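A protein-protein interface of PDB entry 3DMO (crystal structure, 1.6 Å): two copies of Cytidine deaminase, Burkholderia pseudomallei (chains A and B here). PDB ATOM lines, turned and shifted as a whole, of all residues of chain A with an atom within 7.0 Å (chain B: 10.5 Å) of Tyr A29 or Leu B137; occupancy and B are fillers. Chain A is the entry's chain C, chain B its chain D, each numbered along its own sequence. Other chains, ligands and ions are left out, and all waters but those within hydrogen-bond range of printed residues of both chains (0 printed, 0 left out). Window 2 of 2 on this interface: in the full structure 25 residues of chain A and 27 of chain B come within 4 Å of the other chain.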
ATOM      1  N   TYR A  26      -1.573  29.461  29.131  1.00  0.00           N
ATOM      2  CA  TYR A  26      -2.615  28.693  28.469  1.00  0.00           C
ATOM      3  C   TYR A  26      -1.960  27.553  27.703  1.00  0.00           C
ATOM      4  O   TYR A  26      -1.463  27.741  26.587  1.00  0.00           O
ATOM      5  CB  TYR A  26      -3.451  29.588  27.545  1.00  0.00           C
ATOM      6  CG  TYR A  26      -4.483  28.844  26.714  1.00  0.00           C
ATOM      7  CD1 TYR A  26      -5.641  28.326  27.298  1.00  0.00           C
ATOM      8  CD2 TYR A  26      -4.307  28.679  25.338  1.00  0.00           C
ATOM      9  CE1 TYR A  26      -6.594  27.645  26.534  1.00  0.00           C
ATOM     10  CE2 TYR A  26      -5.255  27.999  24.563  1.00  0.00           C
ATOM     11  CZ  TYR A  26      -6.389  27.494  25.167  1.00  0.00           C
ATOM     12  OH  TYR A  26      -7.312  26.834  24.392  1.00  0.00           O
ATOM     13  N   ALA A  27      -1.950  26.376  28.323  1.00  0.00           N
ATOM     14  CA  ALA A  27      -1.239  25.224  27.780  1.00  0.00           C
ATOM     15  C   ALA A  27      -2.051  23.929  27.863  1.00  0.00           C
ATOM     16  O   ALA A  27      -1.558  22.924  28.391  1.00  0.00           O
ATOM     17  CB  ALA A  27       0.125  25.058  28.482  1.00  0.00           C
ATOM     18  N   PRO A  28      -3.281  23.925  27.307  1.00  0.00           N
ATOM     19  CA  PRO A  28      -4.110  22.731  27.491  1.00  0.00           C
ATOM     20  C   PRO A  28      -3.645  21.522  26.678  1.00  0.00           C
ATOM     21  O   PRO A  28      -4.081  20.413  26.969  1.00  0.00           O
ATOM     22  CB  PRO A  28      -5.495  23.189  27.023  1.00  0.00           C
ATOM     23  CG  PRO A  28      -5.208  24.227  25.995  1.00  0.00           C
ATOM     24  CD  PRO A  28      -3.968  24.945  26.487  1.00  0.00           C
ATOM     25  N   TYR A  29      -2.766  21.736  25.694  1.00  0.00           N
ATOM     26  CA  TYR A  29      -2.314  20.668  24.797  1.00  0.00           C
ATOM     27  C   TYR A  29      -1.104  19.918  25.342  1.00  0.00           C
ATOM     28  O   TYR A  29      -1.100  18.687  25.353  1.00  0.00           O
ATOM     29  CB  TYR A  29      -2.069  21.208  23.374  1.00  0.00           C
ATOM     30  CG  TYR A  29      -3.289  21.934  22.844  1.00  0.00           C
ATOM     31  CD1 TYR A  29      -3.356  23.326  22.858  1.00  0.00           C
ATOM     32  CD2 TYR A  29      -4.405  21.227  22.388  1.00  0.00           C
ATOM     33  CE1 TYR A  29      -4.491  23.998  22.405  1.00  0.00           C
ATOM     34  CE2 TYR A  29      -5.546  21.892  21.933  1.00  0.00           C
ATOM     35  CZ  TYR A  29      -5.578  23.283  21.949  1.00  0.00           C
ATOM     36  OH  TYR A  29      -6.702  23.954  21.504  1.00  0.00           O
ATOM     37  N   SER A  30      -0.091  20.654  25.799  1.00  0.00           N
ATOM     38  CA  SER A  30       1.093  20.056  26.433  1.00  0.00           C
ATOM     39  C   SER A  30       0.921  19.860  27.941  1.00  0.00           C
ATOM     40  O   SER A  30       1.660  19.079  28.556  1.00  0.00           O
ATOM     41  CB  SER A  30       2.319  20.928  26.211  1.00  0.00           C
ATOM     42  OG  SER A  30       2.191  22.139  26.938  1.00  0.00           O
ATOM     43  N   ASN A  31      -0.015  20.605  28.532  1.00  0.00           N
ATOM     44  CA  ASN A  31      -0.188  20.655  29.989  1.00  0.00           C
ATOM     45  C   ASN A  31       1.088  21.104  30.702  1.00  0.00           C
ATOM     46  O   ASN A  31       1.321  20.761  31.858  1.00  0.00           O
ATOM     47  CB  ASN A  31      -0.698  19.310  30.530  1.00  0.00           C
ATOM     48  CG  ASN A  31      -2.090  18.977  30.028  1.00  0.00           C
ATOM     49  OD1 ASN A  31      -3.043  19.712  30.282  1.00  0.00           O
ATOM     50  ND2 ASN A  31      -2.218  17.862  29.309  1.00  0.00           N
ATOM     51  N   PHE A  32       1.905  21.885  29.997  1.00  0.00           N
ATOM     52  CA  PHE A  32       3.213  22.296  30.482  1.00  0.00           C
ATOM     53  C   PHE A  32       3.316  23.820  30.490  1.00  0.00           C
ATOM     54  O   PHE A  32       3.536  24.445  29.444  1.00  0.00           O
ATOM     55  CB  PHE A  32       4.306  21.693  29.602  1.00  0.00           C
ATOM     56  CG  PHE A  32       5.688  21.865  30.154  1.00  0.00           C
ATOM     57  CD1 PHE A  32       6.141  21.049  31.194  1.00  0.00           C
ATOM     58  CD2 PHE A  32       6.544  22.836  29.635  1.00  0.00           C
ATOM     59  CE1 PHE A  32       7.423  21.204  31.713  1.00  0.00           C
ATOM     60  CE2 PHE A  32       7.836  22.998  30.149  1.00  0.00           C
ATOM     61  CZ  PHE A  32       8.272  22.181  31.187  1.00  0.00           C
ATOM     62  N   GLU A  52      -0.808  28.407  23.960  1.00  0.00           N
ATOM     63  CA  GLU A  52      -0.887  27.359  22.953  1.00  0.00           C
ATOM     64  C   GLU A  52      -2.087  27.513  22.019  1.00  0.00           C
ATOM     65  O   GLU A  52      -2.957  28.358  22.245  1.00  0.00           O
ATOM     66  CB  GLU A  52      -0.853  25.987  23.624  1.00  0.00           C
ATOM     67  CG  GLU A  52       0.451  25.760  24.378  1.00  0.00           C
ATOM     68  CD  GLU A  52       0.585  24.366  24.965  1.00  0.00           C
ATOM     69  OE1 GLU A  52       1.723  24.005  25.323  1.00  0.00           O
ATOM     70  OE2 GLU A  52      -0.434  23.655  25.103  1.00  0.00           O
ATOM     71  N   ASN A  53      -2.109  26.708  20.958  1.00  0.00           N
ATOM     72  CA  ASN A  53      -3.168  26.755  19.966  1.00  0.00           C
ATOM     73  C   ASN A  53      -3.366  25.358  19.416  1.00  0.00           C
ATOM     74  O   ASN A  53      -2.418  24.572  19.363  1.00  0.00           O
ATOM     75  CB  ASN A  53      -2.793  27.726  18.839  1.00  0.00           C
ATOM     76  CG  ASN A  53      -3.949  28.003  17.902  1.00  0.00           C
ATOM     77  OD1 ASN A  53      -4.209  27.242  16.973  1.00  0.00           O
ATOM     78  ND2 ASN A  53      -4.661  29.094  18.152  1.00  0.00           N
ATOM     79  N   ALA A  54      -4.596  25.050  19.029  1.00  0.00           N
ATOM     80  CA  ALA A  54      -4.925  23.759  18.404  1.00  0.00           C
ATOM     81  C   ALA A  54      -4.035  23.474  17.197  1.00  0.00           C
ATOM     82  O   ALA A  54      -3.684  22.312  16.928  1.00  0.00           O
ATOM     83  CB  ALA A  54      -6.385  23.739  18.004  1.00  0.00           C
ATOM     84  N   SER A  55      -3.691  24.525  16.456  1.00  0.00           N
ATOM     85  CA  SER A  55      -2.659  24.450  15.435  1.00  0.00           C
ATOM     86  C   SER A  55      -1.321  24.676  16.136  1.00  0.00           C
ATOM     87  O   SER A  55      -0.967  25.807  16.474  1.00  0.00           O
ATOM     88  CB  SER A  55      -2.886  25.516  14.361  1.00  0.00           C
ATOM     89  OG  SER A  55      -1.923  25.376  13.325  1.00  0.00           O
ATOM     90  N   TYR A  56      -0.574  23.601  16.361  1.00  0.00           N
ATOM     91  CA  TYR A  56       0.601  23.664  17.241  1.00  0.00           C
ATOM     92  C   TYR A  56       1.626  24.722  16.831  1.00  0.00           C
ATOM     93  O   TYR A  56       2.213  25.363  17.686  1.00  0.00           O
ATOM     94  CB  TYR A  56       1.274  22.288  17.375  1.00  0.00           C
ATOM     95  CG  TYR A  56       0.613  21.324  18.355  1.00  0.00           C
ATOM     96  CD1 TYR A  56       1.303  20.195  18.807  1.00  0.00           C
ATOM     97  CD2 TYR A  56      -0.690  21.534  18.828  1.00  0.00           C
ATOM     98  CE1 TYR A  56       0.718  19.295  19.701  1.00  0.00           C
ATOM     99  CE2 TYR A  56      -1.289  20.635  19.723  1.00  0.00           C
ATOM    100  CZ  TYR A  56      -0.574  19.520  20.153  1.00  0.00           C
ATOM    101  OH  TYR A  56      -1.160  18.636  21.026  1.00  0.00           O
ATOM    102  N   CYS A  59       1.524  28.064  18.538  1.00  0.00           N
ATOM    103  CA  CYS A  59       1.865  28.254  19.954  1.00  0.00           C
ATOM    104  C   CYS A  59       2.914  29.370  20.127  1.00  0.00           C
ATOM    105  O   CYS A  59       3.817  29.519  19.303  1.00  0.00           O
ATOM    106  CB  CYS A  59       2.378  26.958  20.595  1.00  0.00           C
ATOM    107  SG  CYS A  59       1.196  25.575  20.657  1.00  0.00           S
ATOM    108  N   PRO B  77      -9.223  32.421  27.490  1.00  0.00           N
ATOM    109  CA  PRO B  77     -10.094  32.341  26.323  1.00  0.00           C
ATOM    110  C   PRO B  77     -11.553  32.666  26.643  1.00  0.00           C
ATOM    111  O   PRO B  77     -12.107  32.168  27.641  1.00  0.00           O
ATOM    112  CB  PRO B  77      -9.955  30.882  25.886  1.00  0.00           C
ATOM    113  CG  PRO B  77      -8.564  30.537  26.289  1.00  0.00           C
ATOM    114  CD  PRO B  77      -8.341  31.242  27.598  1.00  0.00           C
ATOM    115  N   GLN B 101      -6.703  32.186  13.300  1.00  0.00           N
ATOM    116  CA  GLN B 101      -6.698  30.925  14.039  1.00  0.00           C
ATOM    117  C   GLN B 101      -6.529  31.151  15.543  1.00  0.00           C
ATOM    118  O   GLN B 101      -7.184  30.501  16.369  1.00  0.00           O
ATOM    119  CB  GLN B 101      -5.593  30.014  13.507  1.00  0.00           C
ATOM    120  CG  GLN B 101      -5.640  28.576  14.044  1.00  0.00           C
ATOM    121  CD  GLN B 101      -6.898  27.827  13.618  1.00  0.00           C
ATOM    122  OE1 GLN B 101      -7.198  27.709  12.429  1.00  0.00           O
ATOM    123  NE2 GLN B 101      -7.648  27.327  14.597  1.00  0.00           N
ATOM    124  N   VAL B 102      -5.650  32.088  15.889  1.00  0.00           N
ATOM    125  CA  VAL B 102      -5.415  32.476  17.283  1.00  0.00           C
ATOM    126  C   VAL B 102      -6.621  33.247  17.845  1.00  0.00           C
ATOM    127  O   VAL B 102      -7.076  32.976  18.962  1.00  0.00           O
ATOM    128  CB  VAL B 102      -4.107  33.271  17.422  1.00  0.00           C
ATOM    129  CG1 VAL B 102      -3.976  33.878  18.807  1.00  0.00           C
ATOM    130  CG2 VAL B 102      -2.909  32.373  17.126  1.00  0.00           C
ATOM    131  N   ILE B 104      -9.703  32.933  16.913  1.00  0.00           N
ATOM    132  CA  ILE B 104     -10.856  32.070  17.113  1.00  0.00           C
ATOM    133  C   ILE B 104     -10.716  31.229  18.397  1.00  0.00           C
ATOM    134  O   ILE B 104     -11.687  31.077  19.135  1.00  0.00           O
ATOM    135  CB  ILE B 104     -11.249  31.251  15.847  1.00  0.00           C
ATOM    136  CG1 ILE B 104     -12.775  31.036  15.845  1.00  0.00           C
ATOM    137  CG2 ILE B 104     -10.471  29.945  15.765  1.00  0.00           C
ATOM    138  CD1 ILE B 104     -13.360  30.706  14.511  1.00  0.00           C
ATOM    139  N   GLU B 105      -9.505  30.742  18.679  1.00  0.00           N
ATOM    140  CA  GLU B 105      -9.239  29.975  19.898  1.00  0.00           C
ATOM    141  C   GLU B 105      -9.319  30.818  21.183  1.00  0.00           C
ATOM    142  O   GLU B 105      -9.942  30.401  22.168  1.00  0.00           O
ATOM    143  CB  GLU B 105      -7.896  29.241  19.798  1.00  0.00           C
ATOM    144  CG  GLU B 105      -7.494  28.525  21.081  1.00  0.00           C
ATOM    145  CD  GLU B 105      -6.913  27.151  20.838  1.00  0.00           C
ATOM    146  OE1 GLU B 105      -6.686  26.794  19.665  1.00  0.00           O
ATOM    147  OE2 GLU B 105      -6.682  26.431  21.830  1.00  0.00           O
ATOM    148  N   LEU B 106      -8.701  31.998  21.173  1.00  0.00           N
ATOM    149  CA  LEU B 106      -8.651  32.842  22.361  1.00  0.00           C
ATOM    150  C   LEU B 106      -9.892  33.733  22.536  1.00  0.00           C
ATOM    151  O   LEU B 106     -10.325  33.969  23.658  1.00  0.00           O
ATOM    152  CB  LEU B 106      -7.366  33.678  22.374  1.00  0.00           C
ATOM    153  CG  LEU B 106      -6.048  32.889  22.334  1.00  0.00           C
ATOM    154  CD1 LEU B 106      -4.866  33.842  22.313  1.00  0.00           C
ATOM    155  CD2 LEU B 106      -5.937  31.908  23.522  1.00  0.00           C
ATOM    156  N   LYS B 108     -12.964  33.175  20.788  1.00  0.00           N
ATOM    157  CA  LYS B 108     -14.145  32.385  20.390  1.00  0.00           C
ATOM    158  C   LYS B 108     -14.772  32.952  19.101  1.00  0.00           C
ATOM    159  O   LYS B 108     -14.552  34.126  18.768  1.00  0.00           O
ATOM    160  CB  LYS B 108     -15.196  32.284  21.516  1.00  0.00           C
ATOM    161  CG  LYS B 108     -14.654  31.919  22.892  1.00  0.00           C
ATOM    162  CD  LYS B 108     -14.234  30.471  23.008  1.00  0.00           C
ATOM    163  CE  LYS B 108     -13.972  30.134  24.470  1.00  0.00           C
ATOM    164  NZ  LYS B 108     -13.639  28.694  24.667  1.00  0.00           N
ATOM    165  N   ASP B 133     -15.787  27.325   9.271  1.00  0.00           N
ATOM    166  CA  ASP B 133     -15.468  25.933   9.561  1.00  0.00           C
ATOM    167  C   ASP B 133     -14.024  25.819  10.059  1.00  0.00           C
ATOM    168  O   ASP B 133     -13.202  25.130   9.454  1.00  0.00           O
ATOM    169  CB  ASP B 133     -15.708  25.056   8.322  1.00  0.00           C
ATOM    170  CG  ASP B 133     -17.150  25.125   7.819  1.00  0.00           C
ATOM    171  OD1 ASP B 133     -17.354  25.473   6.638  1.00  0.00           O
ATOM    172  OD2 ASP B 133     -18.080  24.840   8.605  1.00  0.00           O
ATOM    173  N   ALA B 134     -13.729  26.512  11.158  1.00  0.00           N
ATOM    174  CA  ALA B 134     -12.379  26.564  11.720  1.00  0.00           C
ATOM    175  C   ALA B 134     -11.897  25.229  12.266  1.00  0.00           C
ATOM    176  O   ALA B 134     -12.693  24.421  12.749  1.00  0.00           O
ATOM    177  CB  ALA B 134     -12.293  27.638  12.801  1.00  0.00           C
ATOM    178  N   PHE B 135     -10.587  25.011  12.186  1.00  0.00           N
ATOM    179  CA  PHE B 135      -9.943  23.849  12.796  1.00  0.00           C
ATOM    180  C   PHE B 135      -9.950  23.975  14.320  1.00  0.00           C
ATOM    181  O   PHE B 135      -9.613  25.030  14.866  1.00  0.00           O
ATOM    182  CB  PHE B 135      -8.500  23.707  12.291  1.00  0.00           C
ATOM    183  CG  PHE B 135      -7.725  22.592  12.951  1.00  0.00           C
ATOM    184  CD1 PHE B 135      -7.960  21.259  12.611  1.00  0.00           C
ATOM    185  CD2 PHE B 135      -6.754  22.876  13.907  1.00  0.00           C
ATOM    186  CE1 PHE B 135      -7.246  20.230  13.226  1.00  0.00           C
ATOM    187  CE2 PHE B 135      -6.037  21.853  14.526  1.00  0.00           C
ATOM    188  CZ  PHE B 135      -6.280  20.526  14.184  1.00  0.00           C
ATOM    189  N   TYR B 136     -10.345  22.896  14.990  1.00  0.00           N
ATOM    190  CA  TYR B 136     -10.258  22.793  16.446  1.00  0.00           C
ATOM    191  C   TYR B 136      -9.654  21.453  16.810  1.00  0.00           C
ATOM    192  O   TYR B 136      -9.729  20.497  16.035  1.00  0.00           O
ATOM    193  CB  TYR B 136     -11.641  22.862  17.100  1.00  0.00           C
ATOM    194  CG  TYR B 136     -12.333  24.200  17.039  1.00  0.00           C
ATOM    195  CD1 TYR B 136     -11.910  25.268  17.843  1.00  0.00           C
ATOM    196  CD2 TYR B 136     -13.439  24.389  16.209  1.00  0.00           C
ATOM    197  CE1 TYR B 136     -12.562  26.502  17.796  1.00  0.00           C
ATOM    198  CE2 TYR B 136     -14.095  25.617  16.157  1.00  0.00           C
ATOM    199  CZ  TYR B 136     -13.651  26.661  16.952  1.00  0.00           C
ATOM    200  OH  TYR B 136     -14.298  27.864  16.901  1.00  0.00           O
ATOM    201  N   LEU B 137      -9.070  21.388  18.001  1.00  0.00           N
ATOM    202  CA  LEU B 137      -8.634  20.128  18.578  1.00  0.00           C
ATOM    203  C   LEU B 137      -9.288  20.011  19.960  1.00  0.00           C
ATOM    204  O   LEU B 137      -8.958  20.769  20.878  1.00  0.00           O
ATOM    205  CB  LEU B 137      -7.106  20.076  18.651  1.00  0.00           C
ATOM    206  CG  LEU B 137      -6.420  18.708  18.641  1.00  0.00           C
ATOM    207  CD1 LEU B 137      -6.574  17.988  17.293  1.00  0.00           C
ATOM    208  CD2 LEU B 137      -4.953  18.874  19.008  1.00  0.00           C
ATOM    209  N   ALA B 138     -10.245  19.087  20.081  1.00  0.00           N
ATOM    210  CA  ALA B 138     -11.081  18.946  21.282  1.00  0.00           C
ATOM    211  C   ALA B 138     -10.305  18.429  22.494  1.00  0.00           C
ATOM    212  O   ALA B 138      -9.427  17.569  22.361  1.00  0.00           O
ATOM    213  CB  ALA B 138     -12.259  18.041  20.991  1.00  0.00           C
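OH of Tyr A26 is in hydrogen-bond range of OE2 of Glu B105 (2.7 Å). The side-chain hydroxyl (OH) of Tyr A29 is in hydrogen-bond range of the side-chain carboxylate (OE2) of Glu B105 (2.5 Å). The backbone carbonyl oxygen of Gln B101 is in hydrogen-bond range of the side-chain amide nitrogen of Asn A53 (3.4 Å). The side-chain amide nitrogen (ND2) of Asn A53 is in hydrogen-bond range of the side-chain carboxylate (OE1) of Glu B105. N of Ala A54 is in hydrogen-bond range of OE1 of Glu B105, at 2.8 Å.
The backbone carbonyl oxygen of Tyr A26 is in hydrogen-bond range of the backbone NH of Glu A52 (2.8 Å). The side-chain carboxylate (OE2) of Glu A52 is in hydrogen-bond range of the backbone NH (N) of Tyr A29. The backbone NH of Ala A54 lies within hydrogen-bond range of the side-chain hydroxyl of Tyr A29 (3.4 Å). The side-chain amide oxygen of Asn A53 lies within hydrogen-bond range of the backbone NH of Ser A55 (2.8 Å). N of Asn A53 sits at hydrogen-bond distance from SG of Cys A59, 3.5 Å away. The backbone carbonyl oxygen (O) of Phe B135 lies within hydrogen-bond range of the side-chain amide nitrogen (NE2) of Gln B101, at 3.0 Å.
Among the printed residues, merely in contact across the chains: Tyr A26 with Pro B77, Tyr A29 with Leu B137, Asn A53 with Val B102, Ala A54 with Phe B135 and Ala A54 with Leu B137.
Tyr A29 touches just these residues of chain B: Glu B105 (2.5 Å) and Leu B137 (3.7 Å). No residue of chain B comes within 4 Å of Ala A27. Pro A28 touches none of the printed residues of chain B. Ser A30 touches none of the printed residues of chain B. Of chain B, only Glu B105 (2.8 Å), Phe B135 (3.4 Å) and Leu B137 (3.6 Å) come within 4 Å of Ala A54. Of the printed residues of chain A, Gln B101 touches Asn A53. Of the printed residues of chain B, Asn A53 touches Gln B101 (3.4 Å), Val B102 (3.6 Å) and Glu B105 (3.4 Å). Printed residues of chain A within 4 Å of Phe B135: Ala A54. Leu B106 touches none of the printed residues of chain A. Ile B104 touches none of the printed residues of chain A. The nearest printed residue of chain A that does not touch Phe B135 is Ser A55 (4.05 Å).
Hydrophobic or aromatic side chains of chain A that line the printed part of chain B: Tyr A26, Tyr A29 and Ala A54. Of the 13 printed residues of chain B, 6 touch a printed residue of chain A. Hydrophobic or aromatic side chains of chain B within 4 Å of the printed part of chain A: Pro B77, Val B102, Phe B135 and Leu B137. Among the printed residues, 10 pairs touch across the chains.
No position is printed for both chains.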
